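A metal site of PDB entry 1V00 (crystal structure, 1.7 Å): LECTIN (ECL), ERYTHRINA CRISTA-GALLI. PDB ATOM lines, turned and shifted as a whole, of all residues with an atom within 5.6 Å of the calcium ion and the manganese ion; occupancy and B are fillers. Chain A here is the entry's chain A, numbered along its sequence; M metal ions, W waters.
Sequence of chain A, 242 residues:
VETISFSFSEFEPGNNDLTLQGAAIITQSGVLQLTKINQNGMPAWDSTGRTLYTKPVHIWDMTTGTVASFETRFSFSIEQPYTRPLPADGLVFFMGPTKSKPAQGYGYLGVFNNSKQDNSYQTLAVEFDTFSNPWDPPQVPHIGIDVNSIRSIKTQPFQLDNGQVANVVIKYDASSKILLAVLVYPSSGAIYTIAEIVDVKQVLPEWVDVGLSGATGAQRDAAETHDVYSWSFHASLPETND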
ATOM      1  N   ASP A  89      -1.734   0.292  30.114  1.00  0.00           N
ATOM      2  CA  ASP A  89      -2.678  -0.521  29.351  1.00  0.00           C
ATOM      3  C   ASP A  89      -3.994   0.222  29.107  1.00  0.00           C
ATOM      4  O   ASP A  89      -4.738  -0.105  28.185  1.00  0.00           O
ATOM      5  CB  ASP A  89      -2.983  -1.836  30.107  1.00  0.00           C
ATOM      6  CG  ASP A  89      -2.104  -2.990  29.664  1.00  0.00           C
ATOM      7  OD1 ASP A  89      -1.147  -3.328  30.392  1.00  0.00           O
ATOM      8  OD2 ASP A  89      -2.378  -3.546  28.581  1.00  0.00           O
ATOM      9  N   GLY A 107      -3.763  -5.878  30.509  1.00  0.00           N
ATOM     10  CA  GLY A 107      -4.865  -5.726  29.565  1.00  0.00           C
ATOM     11  C   GLY A 107      -6.263  -5.919  30.118  1.00  0.00           C
ATOM     12  O   GLY A 107      -7.239  -5.522  29.473  1.00  0.00           O
ATOM     13  N   GLU A 127     -14.207   1.340  28.294  1.00  0.00           N
ATOM     14  CA  GLU A 127     -12.752   1.422  28.364  1.00  0.00           C
ATOM     15  C   GLU A 127     -12.119   2.437  27.440  1.00  0.00           C
ATOM     16  O   GLU A 127     -12.688   2.812  26.412  1.00  0.00           O
ATOM     17  CB  GLU A 127     -12.149   0.051  28.057  1.00  0.00           C
ATOM     18  CG  GLU A 127     -12.506  -0.459  26.667  1.00  0.00           C
ATOM     19  CD  GLU A 127     -11.740  -1.700  26.261  1.00  0.00           C
ATOM     20  OE1 GLU A 127     -11.765  -2.702  27.020  1.00  0.00           O
ATOM     21  OE2 GLU A 127     -11.104  -1.689  25.186  1.00  0.00           O
ATOM     22  N   ASP A 129      -8.734   2.182  26.078  1.00  0.00           N
ATOM     23  CA  ASP A 129      -7.669   1.217  25.885  1.00  0.00           C
ATOM     24  C   ASP A 129      -6.475   1.693  25.077  1.00  0.00           C
ATOM     25  O   ASP A 129      -6.615   2.085  23.920  1.00  0.00           O
ATOM     26  CB  ASP A 129      -8.317   0.004  25.231  1.00  0.00           C
ATOM     27  CG  ASP A 129      -7.495  -1.219  25.337  1.00  0.00           C
ATOM     28  OD1 ASP A 129      -8.044  -2.310  25.050  1.00  0.00           O
ATOM     29  OD2 ASP A 129      -6.302  -1.104  25.699  1.00  0.00           O
ATOM     30  N   THR A 130      -5.285   1.622  25.669  1.00  0.00           N
ATOM     31  CA  THR A 130      -4.085   2.105  25.009  1.00  0.00           C
ATOM     32  C   THR A 130      -3.119   1.077  24.443  1.00  0.00           C
ATOM     33  O   THR A 130      -2.150   1.436  23.764  1.00  0.00           O
ATOM     34  CB  THR A 130      -3.291   3.000  25.969  1.00  0.00           C
ATOM     35  OG1 THR A 130      -2.989   2.239  27.156  1.00  0.00           O
ATOM     36  CG2 THR A 130      -4.098   4.237  26.341  1.00  0.00           C
ATOM     37  N   PHE A 131      -3.354  -0.211  24.712  1.00  0.00           N
ATOM     38  CA  PHE A 131      -2.464  -1.251  24.218  1.00  0.00           C
ATOM     39  C   PHE A 131      -3.271  -2.312  23.484  1.00  0.00           C
ATOM     40  O   PHE A 131      -4.247  -2.799  24.005  1.00  0.00           O
ATOM     41  CB  PHE A 131      -1.709  -1.911  25.391  1.00  0.00           C
ATOM     42  CG  PHE A 131      -0.773  -3.004  24.960  1.00  0.00           C
ATOM     43  CD1 PHE A 131       0.551  -2.716  24.626  1.00  0.00           C
ATOM     44  CD2 PHE A 131      -1.228  -4.308  24.832  1.00  0.00           C
ATOM     45  CE1 PHE A 131       1.417  -3.721  24.172  1.00  0.00           C
ATOM     46  CE2 PHE A 131      -0.381  -5.323  24.373  1.00  0.00           C
ATOM     47  CZ  PHE A 131       0.952  -5.025  24.041  1.00  0.00           C
ATOM     48  N   SER A 132      -2.860  -2.679  22.273  1.00  0.00           N
ATOM     49  CA  SER A 132      -3.604  -3.680  21.532  1.00  0.00           C
ATOM     50  C   SER A 132      -3.234  -5.127  21.898  1.00  0.00           C
ATOM     51  O   SER A 132      -2.185  -5.632  21.501  1.00  0.00           O
ATOM     52  CB  SER A 132      -3.404  -3.478  20.021  1.00  0.00           C
ATOM     53  OG  SER A 132      -4.173  -4.418  19.286  1.00  0.00           O
ATOM     54  N   ASN A 133      -4.100  -5.766  22.683  1.00  0.00           N
ATOM     55  CA  ASN A 133      -3.891  -7.159  23.086  1.00  0.00           C
ATOM     56  C   ASN A 133      -4.424  -8.087  22.004  1.00  0.00           C
ATOM     57  O   ASN A 133      -5.052  -7.633  21.053  1.00  0.00           O
ATOM     58  CB  ASN A 133      -4.606  -7.464  24.411  1.00  0.00           C
ATOM     59  CG  ASN A 133      -4.011  -6.706  25.586  1.00  0.00           C
ATOM     60  OD1 ASN A 133      -4.418  -5.588  25.869  1.00  0.00           O
ATOM     61  ND2 ASN A 133      -3.048  -7.312  26.261  1.00  0.00           N
ATOM     62  N   TRP A 135      -6.968  -9.881  21.869  1.00  0.00           N
ATOM     63  CA  TRP A 135      -8.422  -9.809  21.740  1.00  0.00           C
ATOM     64  C   TRP A 135      -8.913  -8.421  21.300  1.00  0.00           C
ATOM     65  O   TRP A 135     -10.110  -8.201  21.142  1.00  0.00           O
ATOM     66  CB  TRP A 135      -9.067 -10.153  23.082  1.00  0.00           C
ATOM     67  CG  TRP A 135      -8.606  -9.241  24.196  1.00  0.00           C
ATOM     68  CD1 TRP A 135      -9.023  -7.958  24.425  1.00  0.00           C
ATOM     69  CD2 TRP A 135      -7.592  -9.511  25.166  1.00  0.00           C
ATOM     70  NE1 TRP A 135      -8.332  -7.414  25.486  1.00  0.00           N
ATOM     71  CE2 TRP A 135      -7.449  -8.354  25.960  1.00  0.00           C
ATOM     72  CE3 TRP A 135      -6.787 -10.624  25.445  1.00  0.00           C
ATOM     73  CZ2 TRP A 135      -6.526  -8.273  27.010  1.00  0.00           C
ATOM     74  CZ3 TRP A 135      -5.874 -10.554  26.493  1.00  0.00           C
ATOM     75  CH2 TRP A 135      -5.756  -9.379  27.266  1.00  0.00           C
ATOM     76  N   ASP A 136      -7.965  -7.517  21.082  1.00  0.00           N
ATOM     77  CA  ASP A 136      -8.284  -6.142  20.698  1.00  0.00           C
ATOM     78  C   ASP A 136      -8.191  -5.826  19.213  1.00  0.00           C
ATOM     79  O   ASP A 136      -7.560  -6.546  18.441  1.00  0.00           O
ATOM     80  CB  ASP A 136      -7.304  -5.153  21.327  1.00  0.00           C
ATOM     81  CG  ASP A 136      -7.585  -4.880  22.769  1.00  0.00           C
ATOM     82  OD1 ASP A 136      -8.752  -4.634  23.105  1.00  0.00           O
ATOM     83  OD2 ASP A 136      -6.615  -4.890  23.549  1.00  0.00           O
ATOM     84  N   PRO A 137      -8.830  -4.717  18.809  1.00  0.00           N
ATOM     85  CA  PRO A 137      -8.780  -4.300  17.415  1.00  0.00           C
ATOM     86  C   PRO A 137      -7.349  -3.767  17.374  1.00  0.00           C
ATOM     87  O   PRO A 137      -6.771  -3.446  18.423  1.00  0.00           O
ATOM     88  CB  PRO A 137      -9.832  -3.183  17.352  1.00  0.00           C
ATOM     89  CG  PRO A 137      -9.846  -2.633  18.745  1.00  0.00           C
ATOM     90  CD  PRO A 137      -9.787  -3.899  19.571  1.00  0.00           C
ATOM     91  N   HIS A 142      -8.311   3.202  21.821  1.00  0.00           N
ATOM     92  CA  HIS A 142      -9.679   3.055  21.353  1.00  0.00           C
ATOM     93  C   HIS A 142     -10.630   3.034  22.528  1.00  0.00           C
ATOM     94  O   HIS A 142     -10.256   2.638  23.644  1.00  0.00           O
ATOM     95  CB  HIS A 142      -9.867   1.763  20.518  1.00  0.00           C
ATOM     96  CG  HIS A 142      -9.512   0.497  21.239  1.00  0.00           C
ATOM     97  ND1 HIS A 142      -8.311  -0.142  21.075  1.00  0.00           N
ATOM     98  CD2 HIS A 142     -10.215  -0.251  22.121  1.00  0.00           C
ATOM     99  CE1 HIS A 142      -8.285  -1.236  21.819  1.00  0.00           C
ATOM    100  NE2 HIS A 142      -9.435  -1.316  22.471  1.00  0.00           N
ATOM    101  N   ILE A 150     -13.667  -8.338  28.400  1.00  0.00           N
ATOM    102  CA  ILE A 150     -12.676  -7.329  28.036  1.00  0.00           C
ATOM    103  C   ILE A 150     -12.675  -7.231  26.504  1.00  0.00           C
ATOM    104  O   ILE A 150     -12.129  -6.278  25.929  1.00  0.00           O
ATOM    105  CB  ILE A 150     -11.272  -7.710  28.553  1.00  0.00           C
ATOM    106  CG1 ILE A 150     -10.283  -6.554  28.342  1.00  0.00           C
ATOM    107  CG2 ILE A 150     -10.760  -8.948  27.822  1.00  0.00           C
ATOM    108  CD1 ILE A 150     -10.550  -5.321  29.195  1.00  0.00           C
ATOM    109  N   SER A 152     -14.453  -6.094  23.869  1.00  0.00           N
ATOM    110  CA  SER A 152     -15.591  -5.203  23.676  1.00  0.00           C
ATOM    111  C   SER A 152     -16.493  -5.550  22.494  1.00  0.00           C
ATOM    112  O   SER A 152     -16.055  -6.060  21.445  1.00  0.00           O
ATOM    113  CB  SER A 152     -15.104  -3.739  23.617  1.00  0.00           C
ATOM    114  OG  SER A 152     -14.427  -3.381  24.810  1.00  0.00           O
ATOM    115  N   THR A 155     -16.020  -0.963  19.428  1.00  0.00           N
ATOM    116  CA  THR A 155     -14.848  -0.124  19.702  1.00  0.00           C
ATOM    117  C   THR A 155     -14.794   1.045  18.733  1.00  0.00           C
ATOM    118  O   THR A 155     -15.382   1.001  17.649  1.00  0.00           O
ATOM    119  CB  THR A 155     -13.526  -0.916  19.605  1.00  0.00           C
ATOM    120  OG1 THR A 155     -13.426  -1.525  18.310  1.00  0.00           O
ATOM    121  CG2 THR A 155     -13.477  -1.994  20.671  1.00  0.00           C
HETATM  122 CA    CA M   1      -5.940  -3.619  25.527  1.00  0.00          CA
HETATM  123 MN    MN M   2      -9.784  -2.979  24.066  1.00  0.00          MN
HETATM  124  O   HOH W   1      -4.562  -2.739  27.490  1.00  0.00           O
HETATM  125  O   HOH W   2      -7.670  -4.758  26.977  1.00  0.00           O
HETATM  126  O   HOH W   3     -10.220  -4.371  25.835  1.00  0.00           O
HETATM  127  O   HOH W   4     -11.503  -3.812  22.970  1.00  0.00           O
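Water W2 lies within hydrogen-bond range of O of Gly 107 and NE1 of Trp 135. Water W3 bridges the side-chain carboxylate of Glu 127 (2.6 Å) and the backbone carbonyl oxygen of Ile 150 (2.7 Å).
The calcium ion is bound by the backbone carbonyl oxygen (O) of Phe 131, the side-chain carboxylate (OD2) of Asp 136, the side-chain amide oxygen (OD1) of Asn 133, the side-chain carboxylate (OD1) of Asp 129, water W2, the side-chain carboxylate (OD2) of Asp 129 and water W1.
Four residues have an atom within 4 Å of the manganese ion: Glu 127, Asp 129, Asp 136 and His 142. The nearest printed residue that does not touch the manganese ion is Ile 150 (4.5 Å).
The manganese ion is bound by OD1 of Asp 129 (2.1 Å), OE2 of Glu 127 (2.2 Å), OD1 of Asp 136 (2.2 Å), water W4 (2.2 Å), water W3 (2.3 Å) and NE2 of His 142 (2.3 Å).
Within 4 Å of the calcium ion: Asp 129, Phe 131, Asn 133 and Asp 136.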
